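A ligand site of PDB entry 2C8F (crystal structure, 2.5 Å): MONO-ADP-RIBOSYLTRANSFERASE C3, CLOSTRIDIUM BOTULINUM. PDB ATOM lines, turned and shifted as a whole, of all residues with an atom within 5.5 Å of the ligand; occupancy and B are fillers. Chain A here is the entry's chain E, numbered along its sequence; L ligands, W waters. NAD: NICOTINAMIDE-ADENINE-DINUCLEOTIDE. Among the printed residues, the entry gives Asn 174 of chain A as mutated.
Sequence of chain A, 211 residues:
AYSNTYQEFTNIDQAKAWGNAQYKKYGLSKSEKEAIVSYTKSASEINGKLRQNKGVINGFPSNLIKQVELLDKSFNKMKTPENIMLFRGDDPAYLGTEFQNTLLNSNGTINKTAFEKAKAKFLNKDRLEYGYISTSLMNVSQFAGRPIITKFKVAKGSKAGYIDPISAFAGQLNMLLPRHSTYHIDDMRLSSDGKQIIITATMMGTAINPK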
ATOM      1  N   TYR A  39      -9.795  19.555 -18.694  1.00  0.00           N
ATOM      2  CA  TYR A  39     -11.174  19.060 -18.678  1.00  0.00           C
ATOM      3  C   TYR A  39     -12.249  20.096 -19.046  1.00  0.00           C
ATOM      4  O   TYR A  39     -13.160  19.779 -19.795  1.00  0.00           O
ATOM      5  CB  TYR A  39     -11.592  18.425 -17.334  1.00  0.00           C
ATOM      6  CG  TYR A  39     -13.064  18.089 -17.380  1.00  0.00           C
ATOM      7  CD1 TYR A  39     -13.542  17.087 -18.204  1.00  0.00           C
ATOM      8  CD2 TYR A  39     -13.995  18.841 -16.647  1.00  0.00           C
ATOM      9  CE1 TYR A  39     -14.901  16.793 -18.283  1.00  0.00           C
ATOM     10  CE2 TYR A  39     -15.351  18.561 -16.717  1.00  0.00           C
ATOM     11  CZ  TYR A  39     -15.801  17.540 -17.529  1.00  0.00           C
ATOM     12  OH  TYR A  39     -17.154  17.258 -17.608  1.00  0.00           O
ATOM     13  N   THR A  40     -12.172  21.310 -18.516  1.00  0.00           N
ATOM     14  CA  THR A  40     -13.206  22.297 -18.790  1.00  0.00           C
ATOM     15  C   THR A  40     -13.108  22.898 -20.176  1.00  0.00           C
ATOM     16  O   THR A  40     -14.077  23.507 -20.620  1.00  0.00           O
ATOM     17  CB  THR A  40     -13.227  23.422 -17.739  1.00  0.00           C
ATOM     18  OG1 THR A  40     -12.041  24.229 -17.892  1.00  0.00           O
ATOM     19  CG2 THR A  40     -13.151  22.859 -16.313  1.00  0.00           C
ATOM     20  N   LYS A  41     -11.961  22.761 -20.833  1.00  0.00           N
ATOM     21  CA  LYS A  41     -11.773  23.229 -22.225  1.00  0.00           C
ATOM     22  C   LYS A  41     -12.395  22.300 -23.253  1.00  0.00           C
ATOM     23  O   LYS A  41     -13.012  22.766 -24.232  1.00  0.00           O
ATOM     24  CB  LYS A  41     -10.288  23.373 -22.572  1.00  0.00           C
ATOM     25  CG  LYS A  41      -9.721  24.754 -22.270  1.00  0.00           C
ATOM     26  CD  LYS A  41      -8.233  24.788 -22.452  1.00  0.00           C
ATOM     27  CE  LYS A  41      -7.665  26.060 -21.892  1.00  0.00           C
ATOM     28  NZ  LYS A  41      -6.208  26.147 -22.123  1.00  0.00           N
ATOM     29  N   ALA A  43     -14.581  19.353 -22.446  1.00  0.00           N
ATOM     30  CA  ALA A  43     -15.402  18.451 -21.615  1.00  0.00           C
ATOM     31  C   ALA A  43     -16.221  17.455 -22.420  1.00  0.00           C
ATOM     32  O   ALA A  43     -16.226  16.271 -22.106  1.00  0.00           O
ATOM     33  CB  ALA A  43     -16.332  19.257 -20.710  1.00  0.00           C
ATOM     34  N   SER A  44     -16.896  17.940 -23.462  1.00  0.00           N
ATOM     35  CA  SER A  44     -17.783  17.084 -24.266  1.00  0.00           C
ATOM     36  C   SER A  44     -17.043  15.983 -25.042  1.00  0.00           C
ATOM     37  O   SER A  44     -17.452  14.833 -25.029  1.00  0.00           O
ATOM     38  CB  SER A  44     -18.668  17.919 -25.181  1.00  0.00           C
ATOM     39  OG  SER A  44     -17.916  18.861 -25.891  1.00  0.00           O
ATOM     40  N   ASN A  47     -16.149  13.226 -22.520  1.00  0.00           N
ATOM     41  CA  ASN A  47     -17.294  12.478 -22.099  1.00  0.00           C
ATOM     42  C   ASN A  47     -17.825  11.772 -23.319  1.00  0.00           C
ATOM     43  O   ASN A  47     -18.007  10.559 -23.311  1.00  0.00           O
ATOM     44  CB  ASN A  47     -18.319  13.421 -21.475  1.00  0.00           C
ATOM     45  CG  ASN A  47     -17.744  14.138 -20.316  1.00  0.00           C
ATOM     46  OD1 ASN A  47     -16.842  13.629 -19.686  1.00  0.00           O
ATOM     47  ND2 ASN A  47     -18.218  15.344 -20.053  1.00  0.00           N
ATOM     48  N   GLY A  48     -18.025  12.547 -24.380  1.00  0.00           N
ATOM     49  CA  GLY A  48     -18.342  12.040 -25.709  1.00  0.00           C
ATOM     50  C   GLY A  48     -17.593  10.755 -26.012  1.00  0.00           C
ATOM     51  O   GLY A  48     -18.188   9.830 -26.544  1.00  0.00           O
ATOM     52  N   ARG A  51     -18.217   7.806 -23.243  1.00  0.00           N
ATOM     53  CA  ARG A  51     -19.526   7.195 -23.442  1.00  0.00           C
ATOM     54  C   ARG A  51     -19.396   6.028 -24.421  1.00  0.00           C
ATOM     55  O   ARG A  51     -19.667   4.878 -24.080  1.00  0.00           O
ATOM     56  CB  ARG A  51     -20.515   8.247 -23.954  1.00  0.00           C
ATOM     57  CG  ARG A  51     -21.926   8.054 -23.472  1.00  0.00           C
ATOM     58  CD  ARG A  51     -22.747   9.324 -23.603  1.00  0.00           C
ATOM     59  NE  ARG A  51     -22.313  10.307 -22.621  1.00  0.00           N
ATOM     60  CZ  ARG A  51     -21.995  11.568 -22.889  1.00  0.00           C
ATOM     61  NH1 ARG A  51     -21.597  12.349 -21.879  1.00  0.00           N
ATOM     62  NH2 ARG A  51     -22.060  12.064 -24.122  1.00  0.00           N
ATOM     63  N   PHE A  87     -27.094  21.916 -10.308  1.00  0.00           N
ATOM     64  CA  PHE A  87     -27.977  22.114 -11.470  1.00  0.00           C
ATOM     65  C   PHE A  87     -27.260  21.854 -12.763  1.00  0.00           C
ATOM     66  O   PHE A  87     -26.044  21.926 -12.855  1.00  0.00           O
ATOM     67  CB  PHE A  87     -28.486  23.555 -11.527  1.00  0.00           C
ATOM     68  CG  PHE A  87     -29.353  23.937 -10.362  1.00  0.00           C
ATOM     69  CD1 PHE A  87     -28.814  24.274  -9.150  1.00  0.00           C
ATOM     70  CD2 PHE A  87     -30.736  23.979 -10.496  1.00  0.00           C
ATOM     71  CE1 PHE A  87     -29.616  24.650  -8.101  1.00  0.00           C
ATOM     72  CE2 PHE A  87     -31.541  24.357  -9.438  1.00  0.00           C
ATOM     73  CZ  PHE A  87     -30.986  24.672  -8.250  1.00  0.00           C
ATOM     74  N   ARG A  88     -28.033  21.638 -13.822  1.00  0.00           N
ATOM     75  CA  ARG A  88     -27.430  21.352 -15.104  1.00  0.00           C
ATOM     76  C   ARG A  88     -28.421  21.513 -16.264  1.00  0.00           C
ATOM     77  O   ARG A  88     -29.500  20.953 -16.228  1.00  0.00           O
ATOM     78  CB  ARG A  88     -26.888  19.928 -15.071  1.00  0.00           C
ATOM     79  CG  ARG A  88     -26.265  19.493 -16.327  1.00  0.00           C
ATOM     80  CD  ARG A  88     -25.930  18.015 -16.394  1.00  0.00           C
ATOM     81  NE  ARG A  88     -25.680  17.648 -17.776  1.00  0.00           N
ATOM     82  CZ  ARG A  88     -24.583  17.975 -18.418  1.00  0.00           C
ATOM     83  NH1 ARG A  88     -23.625  18.636 -17.797  1.00  0.00           N
ATOM     84  NH2 ARG A  88     -24.432  17.645 -19.689  1.00  0.00           N
ATOM     85  N   GLY A  89     -28.057  22.250 -17.300  1.00  0.00           N
ATOM     86  CA  GLY A  89     -28.855  22.286 -18.530  1.00  0.00           C
ATOM     87  C   GLY A  89     -28.455  21.183 -19.497  1.00  0.00           C
ATOM     88  O   GLY A  89     -27.317  20.801 -19.466  1.00  0.00           O
ATOM     89  N   ASP A  90     -29.372  20.682 -20.317  1.00  0.00           N
ATOM     90  CA  ASP A  90     -29.089  19.602 -21.293  1.00  0.00           C
ATOM     91  C   ASP A  90     -29.934  19.868 -22.580  1.00  0.00           C
ATOM     92  O   ASP A  90     -31.037  20.413 -22.485  1.00  0.00           O
ATOM     93  CB  ASP A  90     -29.466  18.212 -20.718  1.00  0.00           C
ATOM     94  CG  ASP A  90     -28.307  17.525 -19.939  1.00  0.00           C
ATOM     95  OD1 ASP A  90     -27.437  16.846 -20.554  1.00  0.00           O
ATOM     96  OD2 ASP A  90     -28.197  17.590 -18.698  1.00  0.00           O
ATOM     97  N   ASP A  91     -29.438  19.475 -23.754  1.00  0.00           N
ATOM     98  CA  ASP A  91     -30.221  19.504 -24.988  1.00  0.00           C
ATOM     99  C   ASP A  91     -30.991  18.176 -25.192  1.00  0.00           C
ATOM    100  O   ASP A  91     -30.777  17.210 -24.438  1.00  0.00           O
ATOM    101  CB  ASP A  91     -29.311  19.777 -26.200  1.00  0.00           C
ATOM    102  CG  ASP A  91     -28.487  21.058 -26.047  1.00  0.00           C
ATOM    103  OD1 ASP A  91     -29.088  22.182 -26.109  1.00  0.00           O
ATOM    104  OD2 ASP A  91     -27.263  20.993 -25.780  1.00  0.00           O
ATOM    105  N   ALA A  93     -30.896  15.606 -27.296  1.00  0.00           N
ATOM    106  CA  ALA A  93     -30.183  14.331 -27.516  1.00  0.00           C
ATOM    107  C   ALA A  93     -29.935  13.550 -26.196  1.00  0.00           C
ATOM    108  O   ALA A  93     -29.782  12.317 -26.207  1.00  0.00           O
ATOM    109  CB  ALA A  93     -28.835  14.592 -28.250  1.00  0.00           C
ATOM    110  N   TYR A  94     -29.874  14.281 -25.095  1.00  0.00           N
ATOM    111  CA  TYR A  94     -29.711  13.718 -23.790  1.00  0.00           C
ATOM    112  C   TYR A  94     -30.756  12.630 -23.521  1.00  0.00           C
ATOM    113  O   TYR A  94     -30.453  11.693 -22.860  1.00  0.00           O
ATOM    114  CB  TYR A  94     -29.719  14.822 -22.711  1.00  0.00           C
ATOM    115  CG  TYR A  94     -29.918  14.281 -21.290  1.00  0.00           C
ATOM    116  CD1 TYR A  94     -28.855  13.739 -20.583  1.00  0.00           C
ATOM    117  CD2 TYR A  94     -31.168  14.279 -20.700  1.00  0.00           C
ATOM    118  CE1 TYR A  94     -29.038  13.253 -19.313  1.00  0.00           C
ATOM    119  CE2 TYR A  94     -31.354  13.771 -19.428  1.00  0.00           C
ATOM    120  CZ  TYR A  94     -30.282  13.248 -18.742  1.00  0.00           C
ATOM    121  OH  TYR A  94     -30.452  12.703 -17.470  1.00  0.00           O
ATOM    122  N   ARG A 127     -30.170   5.574 -14.060  1.00  0.00           N
ATOM    123  CA  ARG A 127     -29.476   5.983 -15.253  1.00  0.00           C
ATOM    124  C   ARG A 127     -27.991   6.042 -14.900  1.00  0.00           C
ATOM    125  O   ARG A 127     -27.631   6.584 -13.880  1.00  0.00           O
ATOM    126  CB  ARG A 127     -30.008   7.333 -15.728  1.00  0.00           C
ATOM    127  CG  ARG A 127     -29.157   7.967 -16.808  1.00  0.00           C
ATOM    128  CD  ARG A 127     -29.946   8.774 -17.836  1.00  0.00           C
ATOM    129  NE  ARG A 127     -29.066   9.254 -18.917  1.00  0.00           N
ATOM    130  CZ  ARG A 127     -29.471   9.788 -20.051  1.00  0.00           C
ATOM    131  NH1 ARG A 127     -30.754   9.933 -20.306  1.00  0.00           N
ATOM    132  NH2 ARG A 127     -28.563  10.170 -20.951  1.00  0.00           N
ATOM    133  N   GLU A 129     -24.134   7.250 -15.972  1.00  0.00           N
ATOM    134  CA  GLU A 129     -23.331   8.122 -16.858  1.00  0.00           C
ATOM    135  C   GLU A 129     -21.848   7.801 -16.843  1.00  0.00           C
ATOM    136  O   GLU A 129     -21.245   7.706 -15.794  1.00  0.00           O
ATOM    137  CB  GLU A 129     -23.498   9.609 -16.506  1.00  0.00           C
ATOM    138  CG  GLU A 129     -22.681  10.552 -17.387  1.00  0.00           C
ATOM    139  CD  GLU A 129     -23.127  10.522 -18.846  1.00  0.00           C
ATOM    140  OE1 GLU A 129     -24.329  10.709 -19.134  1.00  0.00           O
ATOM    141  OE2 GLU A 129     -22.270  10.299 -19.708  1.00  0.00           O
ATOM    142  N   TYR A 132     -17.822  12.284 -17.012  1.00  0.00           N
ATOM    143  CA  TYR A 132     -17.879  13.123 -15.836  1.00  0.00           C
ATOM    144  C   TYR A 132     -19.190  13.924 -15.949  1.00  0.00           C
ATOM    145  O   TYR A 132     -19.770  13.962 -17.036  1.00  0.00           O
ATOM    146  CB  TYR A 132     -16.667  14.057 -15.819  1.00  0.00           C
ATOM    147  CG  TYR A 132     -15.378  13.312 -15.626  1.00  0.00           C
ATOM    148  CD1 TYR A 132     -14.563  13.031 -16.705  1.00  0.00           C
ATOM    149  CD2 TYR A 132     -14.988  12.879 -14.374  1.00  0.00           C
ATOM    150  CE1 TYR A 132     -13.369  12.352 -16.551  1.00  0.00           C
ATOM    151  CE2 TYR A 132     -13.793  12.169 -14.215  1.00  0.00           C
ATOM    152  CZ  TYR A 132     -12.992  11.917 -15.334  1.00  0.00           C
ATOM    153  OH  TYR A 132     -11.777  11.275 -15.232  1.00  0.00           O
ATOM    154  N   SER A 134     -20.733  17.801 -15.352  1.00  0.00           N
ATOM    155  CA  SER A 134     -20.416  19.194 -15.047  1.00  0.00           C
ATOM    156  C   SER A 134     -21.714  19.834 -14.562  1.00  0.00           C
ATOM    157  O   SER A 134     -22.768  19.674 -15.178  1.00  0.00           O
ATOM    158  CB  SER A 134     -19.891  19.943 -16.299  1.00  0.00           C
ATOM    159  OG  SER A 134     -18.619  19.447 -16.739  1.00  0.00           O
ATOM    160  N   THR A 135     -21.649  20.532 -13.423  1.00  0.00           N
ATOM    161  CA  THR A 135     -22.823  21.186 -12.880  1.00  0.00           C
ATOM    162  C   THR A 135     -22.458  22.517 -12.276  1.00  0.00           C
ATOM    163  O   THR A 135     -21.289  22.905 -12.301  1.00  0.00           O
ATOM    164  CB  THR A 135     -23.510  20.292 -11.807  1.00  0.00           C
ATOM    165  OG1 THR A 135     -22.616  20.104 -10.706  1.00  0.00           O
ATOM    166  CG2 THR A 135     -23.743  18.870 -12.346  1.00  0.00           C
ATOM    167  N   SER A 136     -23.455  23.192 -11.722  1.00  0.00           N
ATOM    168  CA  SER A 136     -23.350  24.540 -11.213  1.00  0.00           C
ATOM    169  C   SER A 136     -24.088  24.663  -9.875  1.00  0.00           C
ATOM    170  O   SER A 136     -25.114  24.047  -9.699  1.00  0.00           O
ATOM    171  CB  SER A 136     -23.996  25.493 -12.206  1.00  0.00           C
ATOM    172  OG  SER A 136     -23.427  25.361 -13.479  1.00  0.00           O
ATOM    173  N   PHE A 143     -26.520  28.129 -18.873  1.00  0.00           N
ATOM    174  CA  PHE A 143     -27.150  26.847 -19.218  1.00  0.00           C
ATOM    175  C   PHE A 143     -28.612  26.793 -18.888  1.00  0.00           C
ATOM    176  O   PHE A 143     -29.313  25.923 -19.398  1.00  0.00           O
ATOM    177  CB  PHE A 143     -26.403  25.686 -18.544  1.00  0.00           C
ATOM    178  CG  PHE A 143     -24.921  25.778 -18.704  1.00  0.00           C
ATOM    179  CD1 PHE A 143     -24.133  26.298 -17.673  1.00  0.00           C
ATOM    180  CD2 PHE A 143     -24.323  25.393 -19.900  1.00  0.00           C
ATOM    181  CE1 PHE A 143     -22.752  26.411 -17.825  1.00  0.00           C
ATOM    182  CE2 PHE A 143     -22.957  25.498 -20.067  1.00  0.00           C
ATOM    183  CZ  PHE A 143     -22.156  26.012 -19.031  1.00  0.00           C
ATOM    184  N   ARG A 146     -31.254  25.972 -21.825  1.00  0.00           N
ATOM    185  CA  ARG A 146     -31.410  24.701 -22.562  1.00  0.00           C
ATOM    186  C   ARG A 146     -32.748  24.063 -22.174  1.00  0.00           C
ATOM    187  O   ARG A 146     -33.279  24.348 -21.122  1.00  0.00           O
ATOM    188  CB  ARG A 146     -30.264  23.725 -22.265  1.00  0.00           C
ATOM    189  CG  ARG A 146     -28.896  24.365 -22.252  1.00  0.00           C
ATOM    190  CD  ARG A 146     -27.887  23.724 -23.167  1.00  0.00           C
ATOM    191  NE  ARG A 146     -27.071  22.780 -22.417  1.00  0.00           N
ATOM    192  CZ  ARG A 146     -25.757  22.630 -22.533  1.00  0.00           C
ATOM    193  NH1 ARG A 146     -25.024  23.331 -23.395  1.00  0.00           N
ATOM    194  NH2 ARG A 146     -25.158  21.722 -21.772  1.00  0.00           N
ATOM    195  N   GLN A 172     -18.792  31.236 -13.092  1.00  0.00           N
ATOM    196  CA  GLN A 172     -19.982  30.463 -13.495  1.00  0.00           C
ATOM    197  C   GLN A 172     -20.340  29.343 -12.476  1.00  0.00           C
ATOM    198  O   GLN A 172     -21.075  28.411 -12.841  1.00  0.00           O
ATOM    199  CB  GLN A 172     -19.739  29.804 -14.859  1.00  0.00           C
ATOM    200  CG  GLN A 172     -19.958  30.703 -16.091  1.00  0.00           C
ATOM    201  CD  GLN A 172     -19.714  29.981 -17.404  1.00  0.00           C
ATOM    202  OE1 GLN A 172     -19.851  30.572 -18.461  1.00  0.00           O
ATOM    203  NE2 GLN A 172     -19.358  28.696 -17.343  1.00  0.00           N
ATOM    204  N   ASN A 174     -18.988  26.675 -11.188  1.00  0.00           N
ATOM    205  CA  ASN A 174     -18.659  25.356 -11.703  1.00  0.00           C
ATOM    206  C   ASN A 174     -18.318  24.301 -10.653  1.00  0.00           C
ATOM    207  O   ASN A 174     -17.371  24.431  -9.876  1.00  0.00           O
ATOM    208  CB  ASN A 174     -17.455  25.457 -12.660  1.00  0.00           C
ATOM    209  CG  ASN A 174     -17.503  24.433 -13.779  1.00  0.00           C
ATOM    210  OD1 ASN A 174     -18.255  23.438 -13.717  1.00  0.00           O
ATOM    211  ND2 ASN A 174     -16.705  24.656 -14.818  1.00  0.00           N
ATOM    212  N   MET A 175     -19.100  23.226 -10.652  1.00  0.00           N
ATOM    213  CA  MET A 175     -18.822  22.060  -9.829  1.00  0.00           C
ATOM    214  C   MET A 175     -18.563  20.827 -10.727  1.00  0.00           C
ATOM    215  O   MET A 175     -19.096  20.720 -11.811  1.00  0.00           O
ATOM    216  CB  MET A 175     -20.014  21.775  -8.927  1.00  0.00           C
ATOM    217  CG  MET A 175     -20.300  22.841  -7.919  1.00  0.00           C
ATOM    218  SD  MET A 175     -19.090  22.790  -6.621  1.00  0.00           S
ATOM    219  CE  MET A 175     -19.676  21.394  -5.657  1.00  0.00           C
HETATM  220  PA  NAD L   1     -21.500  17.262 -21.801  1.00  0.00           P
HETATM  221  O1A NAD L   1     -22.128  16.916 -20.490  1.00  0.00           O
HETATM  222  O2A NAD L   1     -20.251  16.412 -22.103  1.00  0.00           O
HETATM  223  O5B NAD L   1     -22.627  16.989 -22.942  1.00  0.00           O
HETATM  224  C5B NAD L   1     -22.506  17.541 -24.251  1.00  0.00           C
HETATM  225  C4B NAD L   1     -23.852  17.661 -24.956  1.00  0.00           C
HETATM  226  O4B NAD L   1     -24.329  16.340 -25.100  1.00  0.00           O
HETATM  227  C3B NAD L   1     -24.929  18.394 -24.140  1.00  0.00           C
HETATM  228  O3B NAD L   1     -25.792  19.180 -24.935  1.00  0.00           O
HETATM  229  C2B NAD L   1     -25.764  17.304 -23.519  1.00  0.00           C
HETATM  230  O2B NAD L   1     -27.090  17.670 -23.395  1.00  0.00           O
HETATM  231  C1B NAD L   1     -25.588  16.155 -24.486  1.00  0.00           C
HETATM  232  N9A NAD L   1     -25.617  14.841 -23.834  1.00  0.00           N
HETATM  233  C8A NAD L   1     -25.407  14.535 -22.519  1.00  0.00           C
HETATM  234  N7A NAD L   1     -25.556  13.206 -22.368  1.00  0.00           N
HETATM  235  C5A NAD L   1     -25.856  12.675 -23.552  1.00  0.00           C
HETATM  236  C6A NAD L   1     -26.106  11.376 -23.923  1.00  0.00           C
HETATM  237  N6A NAD L   1     -26.054  10.398 -23.039  1.00  0.00           N
HETATM  238  N1A NAD L   1     -26.409  11.127 -25.242  1.00  0.00           N
HETATM  239  C2A NAD L   1     -26.468  12.155 -26.178  1.00  0.00           C
HETATM  240  N3A NAD L   1     -26.204  13.455 -25.781  1.00  0.00           N
HETATM  241  C4A NAD L   1     -25.897  13.688 -24.490  1.00  0.00           C
HETATM  242  O3  NAD L   1     -21.016  18.828 -21.774  1.00  0.00           O
HETATM  243  PN  NAD L   1     -21.853  20.090 -21.179  1.00  0.00           P
HETATM  244  O1N NAD L   1     -22.155  19.767 -19.790  1.00  0.00           O
HETATM  245  O2N NAD L   1     -22.893  20.444 -22.148  1.00  0.00           O
HETATM  246  O5D NAD L   1     -20.938  21.368 -21.029  1.00  0.00           O
HETATM  247  C5D NAD L   1     -19.582  21.205 -20.685  1.00  0.00           C
HETATM  248  C4D NAD L   1     -18.926  22.593 -20.610  1.00  0.00           C
HETATM  249  O4D NAD L   1     -19.810  23.472 -19.955  1.00  0.00           O
HETATM  250  C3D NAD L   1     -17.676  22.671 -19.763  1.00  0.00           C
HETATM  251  O3D NAD L   1     -17.044  23.907 -20.087  1.00  0.00           O
HETATM  252  C2D NAD L   1     -18.228  22.694 -18.342  1.00  0.00           C
HETATM  253  O2D NAD L   1     -17.353  23.244 -17.394  1.00  0.00           O
HETATM  254  C1D NAD L   1     -19.394  23.624 -18.576  1.00  0.00           C
HETATM  255  N1N NAD L   1     -20.528  23.468 -17.631  1.00  0.00           N
HETATM  256  C2N NAD L   1     -21.748  23.010 -18.077  1.00  0.00           C
HETATM  257  C3N NAD L   1     -22.822  22.889 -17.203  1.00  0.00           C
HETATM  258  C7N NAD L   1     -24.156  22.390 -17.658  1.00  0.00           C
HETATM  259  O7N NAD L   1     -25.138  22.352 -16.714  1.00  0.00           O
HETATM  260  N7N NAD L   1     -24.444  21.994 -18.888  1.00  0.00           N
HETATM  261  C4N NAD L   1     -22.654  23.262 -15.859  1.00  0.00           C
HETATM  262  C5N NAD L   1     -21.401  23.727 -15.425  1.00  0.00           C
HETATM  263  C6N NAD L   1     -20.344  23.833 -16.334  1.00  0.00           C
HETATM  264  O   HOH W   1     -28.570  10.430 -28.172  1.00  0.00           O
HETATM  265  O   HOH W   2     -25.778  24.803 -15.155  1.00  0.00           O
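N6A of the ligand lies close to NH2 of Arg 127, at 3.3 Å. Ala 43 touches the ligand. CA of Ser 44 touches O2A of the ligand, 3.3 Å away. Arg 51 touches the ligand. Phe 87 touches the ligand. Ala 93 touches the ligand. Tyr 94 touches the ligand. Ser 134 touches the ligand (OG to C2D, 3.6 Å). Thr 135 touches the ligand. Ser 136 touches the ligand (OG to C5N, 3.2 Å). Phe 143 touches the ligand. Hydrophobic or aromatic side chains within 4 Å of the ligand: Ala 43, Ala 93, Tyr 94 and Phe 143. Within 4 Å of the ligand: Thr 40, Ala 43, Ser 44, Asn 47, Arg 51, Phe 87, Arg 88, Gly 89, Asp 90, Asp 91, Ala 93, Tyr 94, Arg 127, Ser 134, Thr 135, Ser 136, Phe 143, Arg 146 and Asn 174.
The backbone carbonyl oxygen (O) of Ser 134 sits at hydrogen-bond distance from the guanidinium group (NH1) of Arg 88 (2.9 Å). The guanidinium group (NH2) of Arg 146 lies within hydrogen-bond range of the backbone carbonyl oxygen (O) of Gly 89 (3.3 Å). O of Ala 43 lies within hydrogen-bond range of ND2 of Asn 47. OD1 of Asn 47 sits at hydrogen-bond distance from N of Tyr 132 (3.1 Å). The backbone carbonyl oxygen (O) of Thr 135 sits at hydrogen-bond distance from the backbone NH (N) of Met 175 (2.8 Å). The backbone carbonyl oxygen of Ser 136 lies within hydrogen-bond range of the backbone NH of Phe 87 (3.0 Å). NH2 of Arg 127 is in hydrogen-bond range of O of Tyr 94 (3.1 Å). The side-chain carboxylate (OE2) of Glu 129 lies within salt-bridge range of the guanidinium group (NE) of Arg 51 (2.9 Å).
Water W2 lies within hydrogen-bond range of the side-chain hydroxyl of Ser 136 (2.9 Å) and an oxygen (O7N) of the ligand (3.0 Å).
The backbone NH (N) of Asp 91 sits at hydrogen-bond distance from an oxygen (O2B) of the ligand (3.0 Å). OD2 of Asp 91 lies within hydrogen-bond range of O3B of the ligand (2.5 Å). The guanidinium group (NH2) of Arg 88 is in salt-bridge range of an oxygen (O1A) of the ligand. An oxygen (O2N) of the ligand is in salt-bridge range of the guanidinium group of Arg 146. An oxygen (O7N) of the ligand sits at hydrogen-bond distance from the backbone NH (N) of Gly 89 (3.0 Å). A nitrogen (N7N) of the ligand lies within hydrogen-bond range of the backbone carbonyl oxygen (O) of Gly 89 (3.2 Å). The side-chain carboxylate (OD1) of Asp 90 lies within hydrogen-bond range of an oxygen (O2B) of the ligand, at 3.0 Å. The side-chain amide nitrogen (ND2) of Asn 174 lies within hydrogen-bond range of an oxygen (O2D) of the ligand (3.0 Å). An oxygen (O3D) of the ligand lies within hydrogen-bond range of the backbone carbonyl oxygen (O) of Thr 40. An oxygen (O2A) of the ligand sits at hydrogen-bond distance from the side-chain amide nitrogen (ND2) of Asn 47.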
